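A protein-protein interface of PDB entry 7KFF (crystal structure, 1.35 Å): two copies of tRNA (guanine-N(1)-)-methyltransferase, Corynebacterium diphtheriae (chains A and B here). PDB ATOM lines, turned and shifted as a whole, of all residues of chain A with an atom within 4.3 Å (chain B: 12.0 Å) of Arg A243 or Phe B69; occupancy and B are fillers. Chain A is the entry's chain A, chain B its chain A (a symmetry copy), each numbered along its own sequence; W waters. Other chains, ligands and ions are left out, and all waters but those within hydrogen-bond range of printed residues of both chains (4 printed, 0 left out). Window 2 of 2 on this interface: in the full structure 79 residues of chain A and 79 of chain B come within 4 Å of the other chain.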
ATOM      1  N   TYR A 239     -18.494  16.643  21.093  1.00  0.00           N
ATOM      2  CA  TYR A 239     -19.938  16.768  21.185  1.00  0.00           C
ATOM      3  C   TYR A 239     -20.560  16.575  19.814  1.00  0.00           C
ATOM      4  O   TYR A 239     -19.948  16.907  18.797  1.00  0.00           O
ATOM      5  CB  TYR A 239     -20.333  18.167  21.698  1.00  0.00           C
ATOM      6  CG  TYR A 239     -19.735  18.520  23.029  1.00  0.00           C
ATOM      7  CD1 TYR A 239     -20.385  18.181  24.200  1.00  0.00           C
ATOM      8  CD2 TYR A 239     -18.506  19.154  23.125  1.00  0.00           C
ATOM      9  CE1 TYR A 239     -19.835  18.476  25.431  1.00  0.00           C
ATOM     10  CE2 TYR A 239     -17.953  19.464  24.358  1.00  0.00           C
ATOM     11  CZ  TYR A 239     -18.615  19.120  25.500  1.00  0.00           C
ATOM     12  OH  TYR A 239     -18.063  19.399  26.727  1.00  0.00           O
ATOM     13  N   THR A 240     -21.801  16.079  19.803  1.00  0.00           N
ATOM     14  CA  THR A 240     -22.613  15.983  18.586  1.00  0.00           C
ATOM     15  C   THR A 240     -24.049  16.387  18.913  1.00  0.00           C
ATOM     16  O   THR A 240     -24.369  16.752  20.044  1.00  0.00           O
ATOM     17  CB  THR A 240     -22.466  14.595  17.931  1.00  0.00           C
ATOM     18  OG1 THR A 240     -23.102  14.615  16.644  1.00  0.00           O
ATOM     19  CG2 THR A 240     -23.083  13.511  18.780  1.00  0.00           C
ATOM     20  N   LYS A 241     -24.905  16.336  17.898  1.00  0.00           N
ATOM     21  CA  LYS A 241     -26.294  16.735  18.077  1.00  0.00           C
ATOM     22  C   LYS A 241     -26.964  15.828  19.110  1.00  0.00           C
ATOM     23  O   LYS A 241     -26.625  14.649  19.219  1.00  0.00           O
ATOM     24  CB  LYS A 241     -27.036  16.630  16.751  1.00  0.00           C
ATOM     25  CG  LYS A 241     -26.536  17.596  15.682  1.00  0.00           C
ATOM     26  CD  LYS A 241     -27.294  17.389  14.370  1.00  0.00           C
ATOM     27  CE  LYS A 241     -26.641  18.133  13.218  1.00  0.00           C
ATOM     28  NZ  LYS A 241     -25.359  17.502  12.773  1.00  0.00           N
ATOM     29  N   PRO A 242     -27.945  16.334  19.859  1.00  0.00           N
ATOM     30  CA  PRO A 242     -28.547  17.673  19.752  1.00  0.00           C
ATOM     31  C   PRO A 242     -27.798  18.763  20.526  1.00  0.00           C
ATOM     32  O   PRO A 242     -26.933  18.456  21.368  1.00  0.00           O
ATOM     33  CB  PRO A 242     -29.940  17.458  20.348  1.00  0.00           C
ATOM     34  CG  PRO A 242     -29.705  16.445  21.413  1.00  0.00           C
ATOM     35  CD  PRO A 242     -28.667  15.489  20.837  1.00  0.00           C
ATOM     36  N   ARG A 243     -28.133  20.021  20.243  1.00  0.00           N
ATOM     37  CA  ARG A 243     -27.493  21.135  20.935  1.00  0.00           C
ATOM     38  C   ARG A 243     -27.718  21.067  22.438  1.00  0.00           C
ATOM     39  O   ARG A 243     -26.826  21.415  23.220  1.00  0.00           O
ATOM     40  CB  ARG A 243     -28.019  22.457  20.382  1.00  0.00           C
ATOM     41  CG  ARG A 243     -27.600  22.685  18.958  1.00  0.00           C
ATOM     42  CD  ARG A 243     -27.881  24.098  18.509  1.00  0.00           C
ATOM     43  NE  ARG A 243     -27.278  24.356  17.211  1.00  0.00           N
ATOM     44  CZ  ARG A 243     -27.113  25.565  16.694  1.00  0.00           C
ATOM     45  NH1 ARG A 243     -27.500  26.633  17.371  1.00  0.00           N
ATOM     46  NH2 ARG A 243     -26.555  25.699  15.504  1.00  0.00           N
ATOM     47  N   GLU A 244     -28.905  20.641  22.862  1.00  0.00           N
ATOM     48  CA  GLU A 244     -29.240  20.541  24.277  1.00  0.00           C
ATOM     49  C   GLU A 244     -29.806  19.160  24.548  1.00  0.00           C
ATOM     50  O   GLU A 244     -30.709  18.714  23.837  1.00  0.00           O
ATOM     51  CB  GLU A 244     -30.239  21.636  24.682  1.00  0.00           C
ATOM     52  CG  GLU A 244     -30.609  21.542  26.146  1.00  0.00           C
ATOM     53  CD  GLU A 244     -31.609  22.589  26.621  1.00  0.00           C
ATOM     54  OE1 GLU A 244     -31.630  23.719  26.080  1.00  0.00           O
ATOM     55  OE2 GLU A 244     -32.358  22.282  27.563  1.00  0.00           O
ATOM     56  N   LEU A 248     -28.099  19.715  29.322  1.00  0.00           N
ATOM     57  CA  LEU A 248     -26.694  20.019  29.079  1.00  0.00           C
ATOM     58  C   LEU A 248     -26.540  20.540  27.656  1.00  0.00           C
ATOM     59  O   LEU A 248     -26.870  19.841  26.684  1.00  0.00           O
ATOM     60  CB  LEU A 248     -25.853  18.760  29.306  1.00  0.00           C
ATOM     61  CG  LEU A 248     -25.950  18.216  30.728  1.00  0.00           C
ATOM     62  CD1 LEU A 248     -25.203  16.890  30.825  1.00  0.00           C
ATOM     63  CD2 LEU A 248     -25.391  19.206  31.736  1.00  0.00           C
ATOM     64  N   GLU A 249     -26.003  21.745  27.534  1.00  0.00           N
ATOM     65  CA  GLU A 249     -25.841  22.379  26.238  1.00  0.00           C
ATOM     66  C   GLU A 249     -24.416  22.196  25.737  1.00  0.00           C
ATOM     67  O   GLU A 249     -23.459  22.222  26.515  1.00  0.00           O
ATOM     68  CB  GLU A 249     -26.098  23.879  26.335  1.00  0.00           C
ATOM     69  CG  GLU A 249     -27.510  24.262  26.633  1.00  0.00           C
ATOM     70  CD  GLU A 249     -27.709  25.780  26.587  1.00  0.00           C
ATOM     71  OE1 GLU A 249     -28.416  26.315  27.457  1.00  0.00           O
ATOM     72  OE2 GLU A 249     -27.140  26.436  25.683  1.00  0.00           O
ATOM     73  N   VAL A 250     -24.286  21.998  24.430  1.00  0.00           N
ATOM     74  CA  VAL A 250     -22.944  21.981  23.837  1.00  0.00           C
ATOM     75  C   VAL A 250     -22.347  23.378  23.946  1.00  0.00           C
ATOM     76  O   VAL A 250     -23.087  24.373  23.828  1.00  0.00           O
ATOM     77  CB  VAL A 250     -23.008  21.524  22.378  1.00  0.00           C
ATOM     78  CG1 VAL A 250     -23.726  20.177  22.267  1.00  0.00           C
ATOM     79  CG2 VAL A 250     -23.671  22.595  21.514  1.00  0.00           C
ATOM     80  N   LEU A 254     -18.981  26.266  19.766  1.00  0.00           N
ATOM     81  CA  LEU A 254     -18.977  25.250  18.725  1.00  0.00           C
ATOM     82  C   LEU A 254     -20.080  25.451  17.697  1.00  0.00           C
ATOM     83  O   LEU A 254     -20.000  24.871  16.611  1.00  0.00           O
ATOM     84  CB  LEU A 254     -19.088  23.860  19.346  1.00  0.00           C
ATOM     85  CG  LEU A 254     -17.920  23.491  20.259  1.00  0.00           C
ATOM     86  CD1 LEU A 254     -18.118  22.086  20.840  1.00  0.00           C
ATOM     87  CD2 LEU A 254     -16.582  23.587  19.520  1.00  0.00           C
ATOM     88  N   THR A 255     -21.096  26.255  18.004  1.00  0.00           N
ATOM     89  CA  THR A 255     -22.158  26.567  17.057  1.00  0.00           C
ATOM     90  C   THR A 255     -22.014  27.964  16.463  1.00  0.00           C
ATOM     91  O   THR A 255     -22.947  28.461  15.817  1.00  0.00           O
ATOM     92  CB  THR A 255     -23.526  26.423  17.725  1.00  0.00           C
ATOM     93  OG1 THR A 255     -23.659  27.396  18.764  1.00  0.00           O
ATOM     94  CG2 THR A 255     -23.688  25.037  18.333  1.00  0.00           C
ATOM     95  N   ARG A 266     -10.663  24.501  21.358  1.00  0.00           N
ATOM     96  CA  ARG A 266     -10.155  23.137  21.360  1.00  0.00           C
ATOM     97  C   ARG A 266      -8.813  23.066  22.075  1.00  0.00           C
ATOM     98  O   ARG A 266      -8.557  22.135  22.839  1.00  0.00           O
ATOM     99  CB  ARG A 266     -10.011  22.604  19.934  1.00  0.00           C
ATOM    100  CG  ARG A 266     -11.303  22.435  19.135  1.00  0.00           C
ATOM    101  CD  ARG A 266     -11.056  21.457  17.999  1.00  0.00           C
ATOM    102  NE  ARG A 266     -11.619  21.838  16.704  1.00  0.00           N
ATOM    103  CZ  ARG A 266     -12.832  21.498  16.274  1.00  0.00           C
ATOM    104  NH1 ARG A 266     -13.232  21.879  15.071  1.00  0.00           N
ATOM    105  NH2 ARG A 266     -13.655  20.797  17.045  1.00  0.00           N
ATOM    106  N   ASP B  65     -23.808   7.328  15.781  1.00  0.00           N
ATOM    107  CA  ASP B  65     -22.784   8.360  15.703  1.00  0.00           C
ATOM    108  C   ASP B  65     -23.212   9.441  14.725  1.00  0.00           C
ATOM    109  O   ASP B  65     -24.087   9.233  13.881  1.00  0.00           O
ATOM    110  CB  ASP B  65     -21.420   7.791  15.289  1.00  0.00           C
ATOM    111  CG  ASP B  65     -21.467   7.055  13.969  1.00  0.00           C
ATOM    112  OD1 ASP B  65     -21.891   5.882  13.959  1.00  0.00           O
ATOM    113  OD2 ASP B  65     -21.090   7.646  12.948  1.00  0.00           O
ATOM    114  N   ASP B  66     -22.586  10.608  14.853  1.00  0.00           N
ATOM    115  CA  ASP B  66     -22.948  11.786  14.071  1.00  0.00           C
ATOM    116  C   ASP B  66     -21.756  12.735  14.044  1.00  0.00           C
ATOM    117  O   ASP B  66     -20.799  12.587  14.809  1.00  0.00           O
ATOM    118  CB  ASP B  66     -24.217  12.415  14.680  1.00  0.00           C
ATOM    119  CG  ASP B  66     -24.965  13.347  13.742  1.00  0.00           C
ATOM    120  OD1 ASP B  66     -24.585  13.512  12.561  1.00  0.00           O
ATOM    121  OD2 ASP B  66     -25.974  13.899  14.228  1.00  0.00           O
ATOM    122  N   SER B  67     -21.822  13.716  13.146  1.00  0.00           N
ATOM    123  CA  SER B  67     -20.710  14.633  12.966  1.00  0.00           C
ATOM    124  C   SER B  67     -20.483  15.495  14.206  1.00  0.00           C
ATOM    125  O   SER B  67     -21.426  15.842  14.914  1.00  0.00           O
ATOM    126  CB  SER B  67     -21.001  15.562  11.793  1.00  0.00           C
ATOM    127  OG  SER B  67     -21.047  14.831  10.593  1.00  0.00           O
ATOM    128  N   PRO B  68     -19.234  15.858  14.492  1.00  0.00           N
ATOM    129  CA  PRO B  68     -18.974  16.669  15.683  1.00  0.00           C
ATOM    130  C   PRO B  68     -19.414  18.112  15.506  1.00  0.00           C
ATOM    131  O   PRO B  68     -19.226  18.719  14.444  1.00  0.00           O
ATOM    132  CB  PRO B  68     -17.453  16.605  15.838  1.00  0.00           C
ATOM    133  CG  PRO B  68     -16.954  16.338  14.486  1.00  0.00           C
ATOM    134  CD  PRO B  68     -17.985  15.472  13.811  1.00  0.00           C
ATOM    135  N   PHE B  69     -19.969  18.670  16.578  1.00  0.00           N
ATOM    136  CA  PHE B  69     -20.136  20.114  16.637  1.00  0.00           C
ATOM    137  C   PHE B  69     -18.776  20.792  16.538  1.00  0.00           C
ATOM    138  O   PHE B  69     -17.773  20.303  17.077  1.00  0.00           O
ATOM    139  CB  PHE B  69     -20.803  20.536  17.950  1.00  0.00           C
ATOM    140  CG  PHE B  69     -22.292  20.530  17.901  1.00  0.00           C
ATOM    141  CD1 PHE B  69     -22.986  21.407  17.085  1.00  0.00           C
ATOM    142  CD2 PHE B  69     -23.008  19.662  18.692  1.00  0.00           C
ATOM    143  CE1 PHE B  69     -24.372  21.385  17.058  1.00  0.00           C
ATOM    144  CE2 PHE B  69     -24.380  19.644  18.674  1.00  0.00           C
ATOM    145  CZ  PHE B  69     -25.069  20.505  17.855  1.00  0.00           C
ATOM    146  N   GLY B  70     -18.749  21.926  15.854  1.00  0.00           N
ATOM    147  CA  GLY B  70     -17.528  22.649  15.617  1.00  0.00           C
ATOM    148  C   GLY B  70     -16.876  22.325  14.299  1.00  0.00           C
ATOM    149  O   GLY B  70     -15.846  22.927  13.970  1.00  0.00           O
ATOM    150  N   GLY B  71     -17.453  21.417  13.526  1.00  0.00           N
ATOM    151  CA  GLY B  71     -16.840  21.007  12.297  1.00  0.00           C
ATOM    152  C   GLY B  71     -15.701  20.052  12.585  1.00  0.00           C
ATOM    153  O   GLY B  71     -15.444  19.644  13.723  1.00  0.00           O
ATOM    154  N   GLY B  72     -14.999  19.700  11.527  1.00  0.00           N
ATOM    155  CA  GLY B  72     -13.895  18.793  11.667  1.00  0.00           C
ATOM    156  C   GLY B  72     -14.319  17.373  11.389  1.00  0.00           C
ATOM    157  O   GLY B  72     -15.507  17.022  11.401  1.00  0.00           O
ATOM    158  N   PRO B  73     -13.338  16.525  11.131  1.00  0.00           N
ATOM    159  CA  PRO B  73     -13.627  15.183  10.640  1.00  0.00           C
ATOM    160  C   PRO B  73     -13.966  14.249  11.791  1.00  0.00           C
ATOM    161  O   PRO B  73     -13.866  14.580  12.979  1.00  0.00           O
ATOM    162  CB  PRO B  73     -12.309  14.768   9.985  1.00  0.00           C
ATOM    163  CG  PRO B  73     -11.275  15.427  10.851  1.00  0.00           C
ATOM    164  CD  PRO B  73     -11.893  16.733  11.342  1.00  0.00           C
ATOM    165  N   GLY B  74     -14.375  13.064  11.414  1.00  0.00           N
ATOM    166  CA  GLY B  74     -14.671  12.054  12.389  1.00  0.00           C
ATOM    167  C   GLY B  74     -16.128  12.055  12.773  1.00  0.00           C
ATOM    168  O   GLY B  74     -16.947  12.852  12.306  1.00  0.00           O
ATOM    169  N   MET B  75     -16.440  11.142  13.667  1.00  0.00           N
ATOM    170  CA  MET B  75     -17.795  10.977  14.171  1.00  0.00           C
ATOM    171  C   MET B  75     -17.740  10.845  15.670  1.00  0.00           C
ATOM    172  O   MET B  75     -16.755  10.348  16.204  1.00  0.00           O
ATOM    173  CB  MET B  75     -18.415   9.728  13.542  1.00  0.00           C
ATOM    174  CG  MET B  75     -18.514   9.822  12.022  1.00  0.00           C
ATOM    175  SD  MET B  75     -19.637  11.275  11.351  1.00  0.00           S
ATOM    176  CE  MET B  75     -21.370  10.298  11.430  1.00  0.00           C
ATOM    177  N   VAL B  76     -18.801  11.277  16.328  1.00  0.00           N
ATOM    178  CA  VAL B  76     -18.944  11.237  17.776  1.00  0.00           C
ATOM    179  C   VAL B  76     -20.180  10.418  18.097  1.00  0.00           C
ATOM    180  O   VAL B  76     -21.209  10.559  17.438  1.00  0.00           O
ATOM    181  CB  VAL B  76     -19.096  12.671  18.329  1.00  0.00           C
ATOM    182  CG1 VAL B  76     -19.354  12.671  19.810  1.00  0.00           C
ATOM    183  CG2 VAL B  76     -17.869  13.497  17.986  1.00  0.00           C
ATOM    184  N   MET B  77     -20.085   9.565  19.103  1.00  0.00           N
ATOM    185  CA  MET B  77     -21.247   8.763  19.447  1.00  0.00           C
ATOM    186  C   MET B  77     -22.338   9.541  20.168  1.00  0.00           C
ATOM    187  O   MET B  77     -22.053  10.430  20.981  1.00  0.00           O
ATOM    188  CB  MET B  77     -20.871   7.557  20.276  1.00  0.00           C
ATOM    189  CG  MET B  77     -19.845   6.635  19.621  1.00  0.00           C
ATOM    190  SD  MET B  77     -19.329   5.046  20.539  1.00  0.00           S
ATOM    191  CE  MET B  77     -19.945   3.652  19.366  1.00  0.00           C
ATOM    192  N   LYS B  78     -23.592   9.161  19.866  1.00  0.00           N
ATOM    193  CA  LYS B  78     -24.751  10.003  20.124  1.00  0.00           C
ATOM    194  C   LYS B  78     -25.248   9.883  21.558  1.00  0.00           C
ATOM    195  O   LYS B  78     -25.465   8.762  22.040  1.00  0.00           O
ATOM    196  CB  LYS B  78     -25.905   9.549  19.215  1.00  0.00           C
ATOM    197  CG  LYS B  78     -25.752   9.863  17.745  1.00  0.00           C
ATOM    198  CD  LYS B  78     -26.962   9.323  16.958  1.00  0.00           C
ATOM    199  CE  LYS B  78     -27.196  10.040  15.655  1.00  0.00           C
ATOM    200  NZ  LYS B  78     -28.303   9.421  14.858  1.00  0.00           N
ATOM    201  N   PRO B  79     -25.509  11.003  22.238  1.00  0.00           N
ATOM    202  CA  PRO B  79     -26.123  10.922  23.575  1.00  0.00           C
ATOM    203  C   PRO B  79     -27.497  10.299  23.582  1.00  0.00           C
ATOM    204  O   PRO B  79     -27.856   9.642  24.566  1.00  0.00           O
ATOM    205  CB  PRO B  79     -26.183  12.382  24.056  1.00  0.00           C
ATOM    206  CG  PRO B  79     -25.414  13.156  23.139  1.00  0.00           C
ATOM    207  CD  PRO B  79     -25.157  12.381  21.869  1.00  0.00           C
ATOM    208  N   THR B  80     -28.296  10.500  22.530  1.00  0.00           N
ATOM    209  CA  THR B  80     -29.659   9.972  22.526  1.00  0.00           C
ATOM    210  C   THR B  80     -29.706   8.448  22.420  1.00  0.00           C
ATOM    211  O   THR B  80     -30.769   7.852  22.647  1.00  0.00           O
ATOM    212  CB  THR B  80     -30.484  10.598  21.401  1.00  0.00           C
ATOM    213  OG1 THR B  80     -29.809  10.356  20.158  1.00  0.00           O
ATOM    214  CG2 THR B  80     -30.672  12.118  21.623  1.00  0.00           C
ATOM    215  N   GLU B 170     -14.390   9.199  17.299  1.00  0.00           N
ATOM    216  CA  GLU B 170     -13.787  10.240  18.133  1.00  0.00           C
ATOM    217  C   GLU B 170     -14.096  10.053  19.608  1.00  0.00           C
ATOM    218  O   GLU B 170     -13.536  10.757  20.456  1.00  0.00           O
ATOM    219  CB  GLU B 170     -14.287  11.614  17.696  1.00  0.00           C
ATOM    220  CG  GLU B 170     -13.896  11.979  16.274  1.00  0.00           C
ATOM    221  CD  GLU B 170     -12.401  11.896  16.043  1.00  0.00           C
ATOM    222  OE1 GLU B 170     -11.972  11.081  15.196  1.00  0.00           O
ATOM    223  OE2 GLU B 170     -11.660  12.650  16.713  1.00  0.00           O
ATOM    224  N   GLY B 171     -14.973   9.108  19.930  1.00  0.00           N
ATOM    225  CA  GLY B 171     -15.377   8.866  21.294  1.00  0.00           C
ATOM    226  C   GLY B 171     -16.842   9.164  21.513  1.00  0.00           C
ATOM    227  O   GLY B 171     -17.628   9.270  20.565  1.00  0.00           O
ATOM    228  N   ILE B 172     -17.205   9.327  22.767  1.00  0.00           N
ATOM    229  CA  ILE B 172     -18.585   9.503  23.191  1.00  0.00           C
ATOM    230  C   ILE B 172     -18.810  10.964  23.553  1.00  0.00           C
ATOM    231  O   ILE B 172     -17.977  11.586  24.217  1.00  0.00           O
ATOM    232  CB  ILE B 172     -18.867   8.586  24.400  1.00  0.00           C
ATOM    233  CG1 ILE B 172     -18.636   7.107  24.039  1.00  0.00           C
ATOM    234  CG2 ILE B 172     -20.273   8.825  24.922  1.00  0.00           C
ATOM    235  CD1 ILE B 172     -18.714   6.187  25.226  1.00  0.00           C
ATOM    236  N   ASP B 173     -19.939  11.520  23.123  1.00  0.00           N
ATOM    237  CA  ASP B 173     -20.303  12.887  23.506  1.00  0.00           C
ATOM    238  C   ASP B 173     -20.125  13.055  25.011  1.00  0.00           C
ATOM    239  O   ASP B 173     -20.650  12.272  25.806  1.00  0.00           O
ATOM    240  CB  ASP B 173     -21.768  13.134  23.124  1.00  0.00           C
ATOM    241  CG  ASP B 173     -22.249  14.557  23.387  1.00  0.00           C
ATOM    242  OD1 ASP B 173     -22.314  14.973  24.553  1.00  0.00           O
ATOM    243  OD2 ASP B 173     -22.612  15.240  22.403  1.00  0.00           O
ATOM    244  N   GLN B 174     -19.391  14.097  25.402  1.00  0.00           N
ATOM    245  CA  GLN B 174     -18.983  14.230  26.801  1.00  0.00           C
ATOM    246  C   GLN B 174     -20.171  14.382  27.741  1.00  0.00           C
ATOM    247  O   GLN B 174     -20.072  14.051  28.929  1.00  0.00           O
ATOM    248  CB  GLN B 174     -18.012  15.398  26.951  1.00  0.00           C
ATOM    249  CG  GLN B 174     -17.325  15.440  28.295  1.00  0.00           C
ATOM    250  CD  GLN B 174     -16.368  14.288  28.491  1.00  0.00           C
ATOM    251  OE1 GLN B 174     -15.779  13.793  27.533  1.00  0.00           O
ATOM    252  NE2 GLN B 174     -16.206  13.861  29.740  1.00  0.00           N
ATOM    253  N   ARG B 175     -21.289  14.905  27.246  1.00  0.00           N
ATOM    254  CA  ARG B 175     -22.446  15.061  28.122  1.00  0.00           C
ATOM    255  C   ARG B 175     -22.965  13.723  28.632  1.00  0.00           C
ATOM    256  O   ARG B 175     -23.570  13.668  29.705  1.00  0.00           O
ATOM    257  CB  ARG B 175     -23.561  15.794  27.402  1.00  0.00           C
ATOM    258  CG  ARG B 175     -23.169  17.225  27.092  1.00  0.00           C
ATOM    259  CD  ARG B 175     -24.198  17.878  26.164  1.00  0.00           C
ATOM    260  NE  ARG B 175     -24.194  17.223  24.861  1.00  0.00           N
ATOM    261  CZ  ARG B 175     -25.049  17.494  23.886  1.00  0.00           C
ATOM    262  NH1 ARG B 175     -25.978  18.419  24.072  1.00  0.00           N
ATOM    263  NH2 ARG B 175     -24.932  16.865  22.728  1.00  0.00           N
ATOM    264  N   VAL B 176     -22.725  12.633  27.892  1.00  0.00           N
ATOM    265  CA  VAL B 176     -23.119  11.314  28.365  1.00  0.00           C
ATOM    266  C   VAL B 176     -22.424  11.014  29.676  1.00  0.00           C
ATOM    267  O   VAL B 176     -23.035  10.479  30.612  1.00  0.00           O
ATOM    268  CB  VAL B 176     -22.767  10.244  27.313  1.00  0.00           C
ATOM    269  CG1 VAL B 176     -22.962   8.866  27.902  1.00  0.00           C
ATOM    270  CG2 VAL B 176     -23.592  10.453  26.049  1.00  0.00           C
HETATM  271  O   HOH W   1     -26.783  13.105  16.800  1.00  0.00           O
HETATM  272  O   HOH W   2     -17.044  18.470  19.247  1.00  0.00           O
HETATM  273  O   HOH W   3     -23.425  17.778  14.265  1.00  0.00           O
HETATM  274  O   HOH W   4     -27.689  12.191  20.057  1.00  0.00           O
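NH1 of Arg A266 is in hydrogen-bond range of O of Gly B70. The backbone carbonyl oxygen (O) of Thr A240 is in hydrogen-bond range of the guanidinium group (NH2) of Arg B175 (2.7 Å). The backbone carbonyl oxygen (O) of Pro A242 sits at hydrogen-bond distance from the guanidinium group (NH1) of Arg B175 (2.9 Å). The backbone NH (N) of Phe B69 is in hydrogen-bond range of the backbone carbonyl oxygen (O) of Tyr A239, 2.8 Å away. The backbone carbonyl oxygen (O) of Arg A243 lies within hydrogen-bond range of the guanidinium group (NH1) of Arg B175 (3.2 Å). The backbone NH (N) of Thr A240 sits at hydrogen-bond distance from the side-chain carboxylate (OD2) of Asp B173 (2.8 Å). O of Leu A248 sits at hydrogen-bond distance from NH1 of Arg B175 (3.1 Å). NH1 of Arg A266 lies within hydrogen-bond range of O of Gly B71. The side-chain hydroxyl (OG1) of Thr A240 sits at hydrogen-bond distance from the backbone carbonyl oxygen (O) of Ser B67. OD2 of Asp B66 is in salt-bridge range of NZ of Lys A241 (3.9 Å). N of Gly B70 is in hydrogen-bond range of O of Leu A254 (3.3 Å).
The backbone NH (N) of Met B77 sits at hydrogen-bond distance from the backbone carbonyl oxygen (O) of Gly B171. N of Val A250 sits at hydrogen-bond distance from O of Arg A243. The side-chain carboxylate of Asp B173 lies within salt-bridge range of the guanidinium group of Arg B175. N of Asp B173 is in hydrogen-bond range of O of Met B77 (3.2 Å). SD of Met B75 sits at hydrogen-bond distance from N of Ser B67 (3.7 Å). O of Asp B66 lies within hydrogen-bond range of N of Val B76, at 2.8 Å.
Tyr A239 touches Pro B68. Gln B174 touches Tyr A239. CE2 of Phe B69 touches O of Thr A240, at 3.2 Å. CG2 of Thr A240 touches O of Met B77 (3.9 Å). Phe B69 touches Lys A241 (CE2 to N, 3.4 Å). Arg A243 touches Phe B69 (CG to CZ, 3.5 Å). Arg B175 touches Glu A244. Phe B69 touches Val A250 (CD2 to CG1, 3.7 Å). Val A250 touches Arg B175. Leu A254 touches Phe B69 (CB to CB, 3.99 Å).
Of chain B, only Asp B66 (3.7 Å), Phe B69 (3.4 Å) and Pro B79 (3.8 Å) come within 4 Å of Lys A241. Printed residues of chain B within 4 Å of Arg A243: Phe B69 (3.5 Å) and Arg B175 (3.2 Å). Printed residues of chain B within 4 Å of Glu A244: Arg B175 (3.9 Å). Glu A249 touches none of the printed residues of chain B. Of chain B, only Phe B69 comes within 4 Å of Thr A255. Of the printed residues of chain A, Phe B69 touches Tyr A239 (2.8 Å), Thr A240 (3.2 Å), Lys A241 (3.4 Å), Pro A242 (3.9 Å), Arg A243 (3.5 Å), Val A250 (3.7 Å), Leu A254 (3.99 Å) and Thr A255 (3.9 Å). Printed residues of chain A within 4 Å of Gly B71: Arg A266 (3.4 Å). Gly B72 touches none of the printed residues of chain A. Printed residues of chain A within 4 Å of Asp B173: Tyr A239 and Thr A240. The nearest printed residue of chain B that does not touch Arg A243 is Asp B173 (7.5 Å). The nearest printed residue of chain A that does not touch Phe B69 is Arg A266 (4.1 Å).
Of the 23 printed residues of chain B, 12 touch a printed residue of chain A. Hydrophobic or aromatic side chains of chain B within 4 Å of the printed part of chain A: Pro B68, Phe B69, Val B76 and Pro B79.
No position is printed for both chains.
Water W3 lies within hydrogen-bond range of the side-chain amino group (NZ) of Lys A241 (2.5 Å) and the backbone carbonyl oxygen (O) of Ser B67 (2.9 Å). Water W4 bridges the side-chain hydroxyl (OG1) of Thr B80 (2.8 Å) and the backbone carbonyl oxygen (O) of Lys A241 (2.8 Å). Water W1 lies within hydrogen-bond range of OD2 of Asp B66 (2.8 Å) and O of Lys A241 (2.9 Å). Water W2 lies within hydrogen-bond range of O of Phe B69 (2.9 Å) and N of Tyr A239 (3.0 Å).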
